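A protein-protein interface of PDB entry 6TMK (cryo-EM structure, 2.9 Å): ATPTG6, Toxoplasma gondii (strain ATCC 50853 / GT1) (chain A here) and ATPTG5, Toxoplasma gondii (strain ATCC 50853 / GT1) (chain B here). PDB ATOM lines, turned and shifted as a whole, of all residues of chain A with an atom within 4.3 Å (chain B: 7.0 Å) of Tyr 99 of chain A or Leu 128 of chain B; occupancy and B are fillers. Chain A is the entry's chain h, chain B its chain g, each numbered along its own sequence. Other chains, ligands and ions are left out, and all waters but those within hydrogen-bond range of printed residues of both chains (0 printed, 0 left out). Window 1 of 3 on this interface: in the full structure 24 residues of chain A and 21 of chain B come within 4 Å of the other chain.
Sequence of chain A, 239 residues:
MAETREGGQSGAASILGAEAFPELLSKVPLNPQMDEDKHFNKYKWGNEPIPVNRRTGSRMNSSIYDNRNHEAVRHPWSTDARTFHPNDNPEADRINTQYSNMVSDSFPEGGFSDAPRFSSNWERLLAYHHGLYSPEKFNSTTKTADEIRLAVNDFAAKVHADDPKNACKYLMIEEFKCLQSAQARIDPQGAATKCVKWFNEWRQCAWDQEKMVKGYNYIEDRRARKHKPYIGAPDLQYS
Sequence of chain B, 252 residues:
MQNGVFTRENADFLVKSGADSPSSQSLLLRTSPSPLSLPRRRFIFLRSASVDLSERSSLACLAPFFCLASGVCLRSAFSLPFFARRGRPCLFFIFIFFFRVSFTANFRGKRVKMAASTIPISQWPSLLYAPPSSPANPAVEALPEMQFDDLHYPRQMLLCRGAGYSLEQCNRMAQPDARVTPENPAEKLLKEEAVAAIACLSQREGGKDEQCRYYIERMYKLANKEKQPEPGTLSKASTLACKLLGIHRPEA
Of the 13 printed residues of chain A, 9 touch a printed residue of chain B.
Hydrophobic or aromatic side chains of chain A within 4 Å of the printed part of chain B: Tyr 99, Met 102, Ala 145 and Ile 148.
Along chain A the printed residues that touch a printed residue of chain B span positions 97 to 181.
Among the printed residues, 18 pairs touch across the chains.
Among the printed residues, no Asp or Glu carboxylate lies within 4 Å of a Lys or Arg side-chain nitrogen of the other chain.
NE2 of Gln 183 of chain A lies within hydrogen-bond range of OH of Tyr 99 of chain A (3.1 Å).
The backbone carbonyl oxygen of Ser 181 of chain A is in hydrogen-bond range of the side-chain hydroxyl of Tyr 99 of chain A (2.6 Å).
Leu 127 of chain B touches Thr 97 of chain A.
Pro 132 of chain B touches Gln 98 of chain A.
CE1 of Tyr 99 of chain A touches CE3 of Trp 124 of chain B, at 3.5 Å.
Leu 127 of chain B touches Tyr 99 of chain A (CD2 to N, 3.98 Å).
Val 103 of chain A touches Trp 124 of chain B (CA to CH2, 3.8 Å).
Leu 128 of chain B touches Ala 145 of chain A (CD2 to CB, 3.6 Å).
Ile 148 of chain A touches Leu 128 of chain B.
OH of Tyr 129 of chain B touches O of Arg 149 of chain A, 3.6 Å away.
CE3 of Trp 124 of chain B touches O of Ser 181 of chain A (3.5 Å).
Leu 128 of chain B touches Ser 181 of chain A.
Of the printed residues of chain B, Tyr 99 of chain A touches Trp 124, Leu 127 and Leu 128.
Printed residues of chain A within 4 Å of Leu 128 of chain B: Tyr 99 (3.9 Å), Ala 145 (3.6 Å), Ile 148 (3.8 Å), Arg 149 (2.8 Å) and Ser 181 (3.98 Å).
Of the printed residues of chain A, Met 146 of chain B touches Arg 149 (3.5 Å).
Printed residues of chain A within 4 Å of Leu 127 of chain B: Thr 97 (3.5 Å) and Tyr 99 (3.98 Å).
Of the printed residues of chain A, Pro 125 of chain B touches Ser 181 (3.6 Å).
Printed residues of chain B within 4 Å of Ser 181 of chain A: Trp 124 (3.5 Å), Pro 125 (3.6 Å) and Leu 128 (3.98 Å).
Of the printed residues of chain B, Ile 148 of chain A touches Leu 128 (3.8 Å).
The nearest printed residue of chain B that does not touch Tyr 99 of chain A is Pro 125 of chain B (6.3 Å).
The nearest printed residue of chain A that does not touch Leu 128 of chain B is Gln 98 of chain A (7.2 Å).
The nearest printed residue of chain A that does not touch Pro 125 of chain B is Tyr 99 of chain A (6.3 Å).
The side-chain sulfur (SD) of Met 146 of chain B lies within hydrogen-bond range of the guanidinium group (NE) of Arg 149 of chain A (3.5 Å).
O of Leu 128 of chain B is in hydrogen-bond range of NH1 of Arg 149 of chain A, 2.8 Å away.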
ATOM      1  N   THR A  97     -27.543 -23.363  -8.610  1.00  0.00           N
ATOM      2  CA  THR A  97     -26.287 -22.762  -9.022  1.00  0.00           C
ATOM      3  C   THR A  97     -25.143 -23.158  -8.105  1.00  0.00           C
ATOM      4  O   THR A  97     -24.152 -22.430  -8.002  1.00  0.00           O
ATOM      5  CB  THR A  97     -26.415 -21.243  -9.081  1.00  0.00           C
ATOM      6  OG1 THR A  97     -27.060 -20.761  -7.897  1.00  0.00           O
ATOM      7  CG2 THR A  97     -27.200 -20.826 -10.301  1.00  0.00           C
ATOM      8  N   GLN A  98     -25.266 -24.292  -7.429  1.00  0.00           N
ATOM      9  CA  GLN A  98     -24.169 -24.826  -6.652  1.00  0.00           C
ATOM     10  C   GLN A  98     -23.143 -25.496  -7.560  1.00  0.00           C
ATOM     11  O   GLN A  98     -23.400 -25.802  -8.729  1.00  0.00           O
ATOM     12  CB  GLN A  98     -24.681 -25.830  -5.619  1.00  0.00           C
ATOM     13  CG  GLN A  98     -25.611 -25.254  -4.569  1.00  0.00           C
ATOM     14  CD  GLN A  98     -25.013 -24.100  -3.795  1.00  0.00           C
ATOM     15  OE1 GLN A  98     -25.723 -23.175  -3.407  1.00  0.00           O
ATOM     16  NE2 GLN A  98     -23.707 -24.147  -3.562  1.00  0.00           N
ATOM     17  N   TYR A  99     -21.961 -25.727  -6.990  1.00  0.00           N
ATOM     18  CA  TYR A  99     -20.889 -26.395  -7.714  1.00  0.00           C
ATOM     19  C   TYR A  99     -21.316 -27.769  -8.207  1.00  0.00           C
ATOM     20  O   TYR A  99     -20.907 -28.192  -9.292  1.00  0.00           O
ATOM     21  CB  TYR A  99     -19.660 -26.502  -6.817  1.00  0.00           C
ATOM     22  CG  TYR A  99     -18.408 -26.940  -7.528  1.00  0.00           C
ATOM     23  CD1 TYR A  99     -17.568 -26.021  -8.130  1.00  0.00           C
ATOM     24  CD2 TYR A  99     -18.065 -28.274  -7.596  1.00  0.00           C
ATOM     25  CE1 TYR A  99     -16.433 -26.420  -8.778  1.00  0.00           C
ATOM     26  CE2 TYR A  99     -16.936 -28.680  -8.240  1.00  0.00           C
ATOM     27  CZ  TYR A  99     -16.119 -27.752  -8.833  1.00  0.00           C
ATOM     28  OH  TYR A  99     -14.983 -28.163  -9.480  1.00  0.00           O
ATOM     29  N   SER A 100     -22.151 -28.464  -7.438  1.00  0.00           N
ATOM     30  CA  SER A 100     -22.612 -29.790  -7.833  1.00  0.00           C
ATOM     31  C   SER A 100     -23.268 -29.764  -9.206  1.00  0.00           C
ATOM     32  O   SER A 100     -22.987 -30.612 -10.058  1.00  0.00           O
ATOM     33  CB  SER A 100     -23.597 -30.318  -6.795  1.00  0.00           C
ATOM     34  OG  SER A 100     -23.085 -30.205  -5.484  1.00  0.00           O
ATOM     35  N   ASN A 101     -24.153 -28.797  -9.435  1.00  0.00           N
ATOM     36  CA  ASN A 101     -24.852 -28.689 -10.705  1.00  0.00           C
ATOM     37  C   ASN A 101     -24.058 -27.929 -11.756  1.00  0.00           C
ATOM     38  O   ASN A 101     -24.324 -28.095 -12.950  1.00  0.00           O
ATOM     39  CB  ASN A 101     -26.197 -28.007 -10.481  1.00  0.00           C
ATOM     40  CG  ASN A 101     -27.203 -28.328 -11.554  1.00  0.00           C
ATOM     41  OD1 ASN A 101     -27.336 -29.472 -11.982  1.00  0.00           O
ATOM     42  ND2 ASN A 101     -27.926 -27.312 -11.995  1.00  0.00           N
ATOM     43  N   MET A 102     -23.098 -27.103 -11.347  1.00  0.00           N
ATOM     44  CA  MET A 102     -22.303 -26.362 -12.315  1.00  0.00           C
ATOM     45  C   MET A 102     -21.222 -27.228 -12.946  1.00  0.00           C
ATOM     46  O   MET A 102     -20.899 -27.062 -14.126  1.00  0.00           O
ATOM     47  CB  MET A 102     -21.666 -25.148 -11.645  1.00  0.00           C
ATOM     48  CG  MET A 102     -22.610 -24.010 -11.391  1.00  0.00           C
ATOM     49  SD  MET A 102     -23.125 -23.154 -12.879  1.00  0.00           S
ATOM     50  CE  MET A 102     -24.847 -23.605 -12.886  1.00  0.00           C
ATOM     51  N   VAL A 103     -20.647 -28.151 -12.175  1.00  0.00           N
ATOM     52  CA  VAL A 103     -19.535 -28.953 -12.668  1.00  0.00           C
ATOM     53  C   VAL A 103     -19.971 -29.860 -13.809  1.00  0.00           C
ATOM     54  O   VAL A 103     -19.156 -30.227 -14.663  1.00  0.00           O
ATOM     55  CB  VAL A 103     -18.933 -29.760 -11.505  1.00  0.00           C
ATOM     56  CG1 VAL A 103     -19.812 -30.942 -11.164  1.00  0.00           C
ATOM     57  CG2 VAL A 103     -17.539 -30.196 -11.830  1.00  0.00           C
ATOM     58  N   LYS A 143     -13.935 -34.066  -8.062  1.00  0.00           N
ATOM     59  CA  LYS A 143     -13.883 -33.715  -6.657  1.00  0.00           C
ATOM     60  C   LYS A 143     -15.087 -32.867  -6.287  1.00  0.00           C
ATOM     61  O   LYS A 143     -15.535 -32.017  -7.060  1.00  0.00           O
ATOM     62  CB  LYS A 143     -12.597 -32.962  -6.337  1.00  0.00           C
ATOM     63  CG  LYS A 143     -11.355 -33.785  -6.437  1.00  0.00           C
ATOM     64  CD  LYS A 143     -11.132 -34.546  -5.173  1.00  0.00           C
ATOM     65  CE  LYS A 143     -10.321 -35.791  -5.403  1.00  0.00           C
ATOM     66  NZ  LYS A 143     -10.289 -36.608  -4.173  1.00  0.00           N
ATOM     67  N   ALA A 145     -17.093 -30.081  -3.848  1.00  0.00           N
ATOM     68  CA  ALA A 145     -16.737 -28.776  -3.307  1.00  0.00           C
ATOM     69  C   ALA A 145     -16.113 -28.892  -1.924  1.00  0.00           C
ATOM     70  O   ALA A 145     -15.157 -28.178  -1.606  1.00  0.00           O
ATOM     71  CB  ALA A 145     -17.972 -27.888  -3.263  1.00  0.00           C
ATOM     72  N   ILE A 148     -12.541 -30.038  -2.344  1.00  0.00           N
ATOM     73  CA  ILE A 148     -11.742 -28.939  -2.867  1.00  0.00           C
ATOM     74  C   ILE A 148     -11.401 -27.962  -1.754  1.00  0.00           C
ATOM     75  O   ILE A 148     -10.259 -27.508  -1.631  1.00  0.00           O
ATOM     76  CB  ILE A 148     -12.494 -28.253  -4.021  1.00  0.00           C
ATOM     77  CG1 ILE A 148     -12.596 -29.197  -5.211  1.00  0.00           C
ATOM     78  CG2 ILE A 148     -11.814 -26.971  -4.435  1.00  0.00           C
ATOM     79  CD1 ILE A 148     -13.650 -28.832  -6.191  1.00  0.00           C
ATOM     80  N   ARG A 149     -12.388 -27.621  -0.932  1.00  0.00           N
ATOM     81  CA  ARG A 149     -12.172 -26.645   0.123  1.00  0.00           C
ATOM     82  C   ARG A 149     -11.213 -27.174   1.175  1.00  0.00           C
ATOM     83  O   ARG A 149     -10.357 -26.437   1.673  1.00  0.00           O
ATOM     84  CB  ARG A 149     -13.507 -26.280   0.751  1.00  0.00           C
ATOM     85  CG  ARG A 149     -14.331 -25.382  -0.110  1.00  0.00           C
ATOM     86  CD  ARG A 149     -15.488 -24.830   0.648  1.00  0.00           C
ATOM     87  NE  ARG A 149     -16.530 -25.832   0.845  1.00  0.00           N
ATOM     88  CZ  ARG A 149     -17.698 -25.847   0.217  1.00  0.00           C
ATOM     89  NH1 ARG A 149     -18.007 -24.925  -0.671  1.00  0.00           N
ATOM     90  NH2 ARG A 149     -18.564 -26.806   0.479  1.00  0.00           N
ATOM     91  N   SER A 181     -10.441 -26.307  -8.540  1.00  0.00           N
ATOM     92  CA  SER A 181     -11.796 -26.065  -9.016  1.00  0.00           C
ATOM     93  C   SER A 181     -11.962 -26.516 -10.461  1.00  0.00           C
ATOM     94  O   SER A 181     -13.031 -27.003 -10.844  1.00  0.00           O
ATOM     95  CB  SER A 181     -12.138 -24.587  -8.873  1.00  0.00           C
ATOM     96  OG  SER A 181     -11.513 -23.811  -9.872  1.00  0.00           O
ATOM     97  N   GLN A 183     -10.387 -28.999 -11.769  1.00  0.00           N
ATOM     98  CA  GLN A 183     -10.250 -30.452 -11.841  1.00  0.00           C
ATOM     99  C   GLN A 183      -9.024 -30.840 -12.664  1.00  0.00           C
ATOM    100  O   GLN A 183      -9.105 -31.574 -13.648  1.00  0.00           O
ATOM    101  CB  GLN A 183     -11.511 -31.087 -12.430  1.00  0.00           C
ATOM    102  CG  GLN A 183     -12.782 -30.780 -11.694  1.00  0.00           C
ATOM    103  CD  GLN A 183     -12.913 -31.510 -10.390  1.00  0.00           C
ATOM    104  OE1 GLN A 183     -12.188 -32.464 -10.116  1.00  0.00           O
ATOM    105  NE2 GLN A 183     -13.837 -31.061  -9.567  1.00  0.00           N
ATOM    106  N   GLN B 123     -15.561 -18.483 -12.548  1.00  0.00           N
ATOM    107  CA  GLN B 123     -16.138 -17.915 -11.344  1.00  0.00           C
ATOM    108  C   GLN B 123     -16.331 -18.940 -10.239  1.00  0.00           C
ATOM    109  O   GLN B 123     -16.891 -18.606  -9.193  1.00  0.00           O
ATOM    110  CB  GLN B 123     -17.474 -17.255 -11.675  1.00  0.00           C
ATOM    111  CG  GLN B 123     -17.357 -15.851 -12.203  1.00  0.00           C
ATOM    112  CD  GLN B 123     -18.702 -15.186 -12.399  1.00  0.00           C
ATOM    113  OE1 GLN B 123     -19.742 -15.845 -12.382  1.00  0.00           O
ATOM    114  NE2 GLN B 123     -18.692 -13.871 -12.578  1.00  0.00           N
ATOM    115  N   TRP B 124     -15.877 -20.171 -10.441  1.00  0.00           N
ATOM    116  CA  TRP B 124     -16.094 -21.248  -9.491  1.00  0.00           C
ATOM    117  C   TRP B 124     -15.279 -21.083  -8.215  1.00  0.00           C
ATOM    118  O   TRP B 124     -15.760 -21.442  -7.133  1.00  0.00           O
ATOM    119  CB  TRP B 124     -15.763 -22.593 -10.137  1.00  0.00           C
ATOM    120  CG  TRP B 124     -16.747 -23.018 -11.163  1.00  0.00           C
ATOM    121  CD1 TRP B 124     -17.879 -22.371 -11.518  1.00  0.00           C
ATOM    122  CD2 TRP B 124     -16.691 -24.198 -11.966  1.00  0.00           C
ATOM    123  NE1 TRP B 124     -18.537 -23.064 -12.498  1.00  0.00           N
ATOM    124  CE2 TRP B 124     -17.825 -24.195 -12.788  1.00  0.00           C
ATOM    125  CE3 TRP B 124     -15.793 -25.256 -12.068  1.00  0.00           C
ATOM    126  CZ2 TRP B 124     -18.081 -25.202 -13.700  1.00  0.00           C
ATOM    127  CZ3 TRP B 124     -16.050 -26.251 -12.970  1.00  0.00           C
ATOM    128  CH2 TRP B 124     -17.180 -26.219 -13.776  1.00  0.00           C
ATOM    129  N   PRO B 125     -14.044 -20.583  -8.284  1.00  0.00           N
ATOM    130  CA  PRO B 125     -13.307 -20.353  -7.037  1.00  0.00           C
ATOM    131  C   PRO B 125     -13.995 -19.390  -6.091  1.00  0.00           C
ATOM    132  O   PRO B 125     -13.864 -19.537  -4.871  1.00  0.00           O
ATOM    133  CB  PRO B 125     -11.974 -19.790  -7.533  1.00  0.00           C
ATOM    134  CG  PRO B 125     -11.803 -20.379  -8.861  1.00  0.00           C
ATOM    135  CD  PRO B 125     -13.170 -20.422  -9.457  1.00  0.00           C
ATOM    136  N   SER B 126     -14.723 -18.406  -6.613  1.00  0.00           N
ATOM    137  CA  SER B 126     -15.520 -17.538  -5.762  1.00  0.00           C
ATOM    138  C   SER B 126     -16.816 -18.204  -5.338  1.00  0.00           C
ATOM    139  O   SER B 126     -17.358 -17.884  -4.279  1.00  0.00           O
ATOM    140  CB  SER B 126     -15.812 -16.230  -6.485  1.00  0.00           C
ATOM    141  OG  SER B 126     -16.679 -16.441  -7.577  1.00  0.00           O
ATOM    142  N   LEU B 127     -17.321 -19.123  -6.157  1.00  0.00           N
ATOM    143  CA  LEU B 127     -18.523 -19.862  -5.808  1.00  0.00           C
ATOM    144  C   LEU B 127     -18.278 -20.814  -4.650  1.00  0.00           C
ATOM    145  O   LEU B 127     -19.203 -21.114  -3.888  1.00  0.00           O
ATOM    146  CB  LEU B 127     -19.009 -20.626  -7.032  1.00  0.00           C
ATOM    147  CG  LEU B 127     -20.148 -21.621  -6.884  1.00  0.00           C
ATOM    148  CD1 LEU B 127     -21.384 -20.930  -6.401  1.00  0.00           C
ATOM    149  CD2 LEU B 127     -20.381 -22.279  -8.210  1.00  0.00           C
ATOM    150  N   LEU B 128     -17.049 -21.307  -4.507  1.00  0.00           N
ATOM    151  CA  LEU B 128     -16.769 -22.271  -3.454  1.00  0.00           C
ATOM    152  C   LEU B 128     -16.766 -21.626  -2.077  1.00  0.00           C
ATOM    153  O   LEU B 128     -17.144 -22.269  -1.093  1.00  0.00           O
ATOM    154  CB  LEU B 128     -15.426 -22.935  -3.716  1.00  0.00           C
ATOM    155  CG  LEU B 128     -15.387 -23.828  -4.945  1.00  0.00           C
ATOM    156  CD1 LEU B 128     -13.968 -24.027  -5.383  1.00  0.00           C
ATOM    157  CD2 LEU B 128     -16.030 -25.149  -4.649  1.00  0.00           C
ATOM    158  N   TYR B 129     -16.338 -20.371  -1.985  1.00  0.00           N
ATOM    159  CA  TYR B 129     -16.212 -19.683  -0.711  1.00  0.00           C
ATOM    160  C   TYR B 129     -17.234 -18.573  -0.525  1.00  0.00           C
ATOM    161  O   TYR B 129     -17.267 -17.952   0.540  1.00  0.00           O
ATOM    162  CB  TYR B 129     -14.795 -19.130  -0.557  1.00  0.00           C
ATOM    163  CG  TYR B 129     -13.776 -20.221  -0.375  1.00  0.00           C
ATOM    164  CD1 TYR B 129     -13.436 -20.666   0.886  1.00  0.00           C
ATOM    165  CD2 TYR B 129     -13.162 -20.811  -1.463  1.00  0.00           C
ATOM    166  CE1 TYR B 129     -12.521 -21.663   1.060  1.00  0.00           C
ATOM    167  CE2 TYR B 129     -12.243 -21.812  -1.298  1.00  0.00           C
ATOM    168  CZ  TYR B 129     -11.923 -22.233  -0.032  1.00  0.00           C
ATOM    169  OH  TYR B 129     -11.005 -23.235   0.154  1.00  0.00           O
ATOM    170  N   ALA B 130     -18.065 -18.310  -1.528  1.00  0.00           N
ATOM    171  CA  ALA B 130     -19.198 -17.394  -1.411  1.00  0.00           C
ATOM    172  C   ALA B 130     -20.368 -17.975  -2.187  1.00  0.00           C
ATOM    173  O   ALA B 130     -20.797 -17.425  -3.206  1.00  0.00           O
ATOM    174  CB  ALA B 130     -18.834 -16.002  -1.926  1.00  0.00           C
ATOM    175  N   PRO B 131     -20.912 -19.096  -1.730  1.00  0.00           N
ATOM    176  CA  PRO B 131     -21.951 -19.774  -2.495  1.00  0.00           C
ATOM    177  C   PRO B 131     -23.245 -18.986  -2.474  1.00  0.00           C
ATOM    178  O   PRO B 131     -23.433 -18.104  -1.624  1.00  0.00           O
ATOM    179  CB  PRO B 131     -22.105 -21.115  -1.772  1.00  0.00           C
ATOM    180  CG  PRO B 131     -21.619 -20.872  -0.416  1.00  0.00           C
ATOM    181  CD  PRO B 131     -20.580 -19.814  -0.491  1.00  0.00           C
ATOM    182  N   PRO B 132     -24.161 -19.273  -3.392  1.00  0.00           N
ATOM    183  CA  PRO B 132     -25.444 -18.571  -3.395  1.00  0.00           C
ATOM    184  C   PRO B 132     -26.297 -18.966  -2.202  1.00  0.00           C
ATOM    185  O   PRO B 132     -25.997 -19.898  -1.456  1.00  0.00           O
ATOM    186  CB  PRO B 132     -26.079 -19.017  -4.712  1.00  0.00           C
ATOM    187  CG  PRO B 132     -25.462 -20.328  -4.982  1.00  0.00           C
ATOM    188  CD  PRO B 132     -24.057 -20.205  -4.523  1.00  0.00           C
ATOM    189  N   PRO B 138     -24.493 -22.952   4.471  1.00  0.00           N
ATOM    190  CA  PRO B 138     -23.418 -23.179   5.437  1.00  0.00           C
ATOM    191  C   PRO B 138     -22.929 -21.889   6.069  1.00  0.00           C
ATOM    192  O   PRO B 138     -23.416 -20.803   5.741  1.00  0.00           O
ATOM    193  CB  PRO B 138     -22.331 -23.831   4.582  1.00  0.00           C
ATOM    194  CG  PRO B 138     -22.507 -23.185   3.258  1.00  0.00           C
ATOM    195  CD  PRO B 138     -23.975 -22.896   3.096  1.00  0.00           C
ATOM    196  N   LEU B 143     -16.269 -21.392   6.251  1.00  0.00           N
ATOM    197  CA  LEU B 143     -15.833 -22.277   5.181  1.00  0.00           C
ATOM    198  C   LEU B 143     -14.321 -22.315   4.991  1.00  0.00           C
ATOM    199  O   LEU B 143     -13.813 -23.376   4.591  1.00  0.00           O
ATOM    200  CB  LEU B 143     -16.508 -21.868   3.870  1.00  0.00           C
ATOM    201  CG  LEU B 143     -17.968 -22.257   3.660  1.00  0.00           C
ATOM    202  CD1 LEU B 143     -18.451 -21.699   2.353  1.00  0.00           C
ATOM    203  CD2 LEU B 143     -18.167 -23.749   3.690  1.00  0.00           C
ATOM    204  N   MET B 146     -12.842 -25.130   7.542  1.00  0.00           N
ATOM    205  CA  MET B 146     -13.136 -26.549   7.455  1.00  0.00           C
ATOM    206  C   MET B 146     -11.898 -27.297   6.982  1.00  0.00           C
ATOM    207  O   MET B 146     -11.330 -26.980   5.933  1.00  0.00           O
ATOM    208  CB  MET B 146     -14.321 -26.783   6.523  1.00  0.00           C
ATOM    209  CG  MET B 146     -14.045 -26.521   5.077  1.00  0.00           C
ATOM    210  SD  MET B 146     -15.557 -26.298   4.132  1.00  0.00           S
ATOM    211  CE  MET B 146     -15.928 -27.995   3.742  1.00  0.00           C
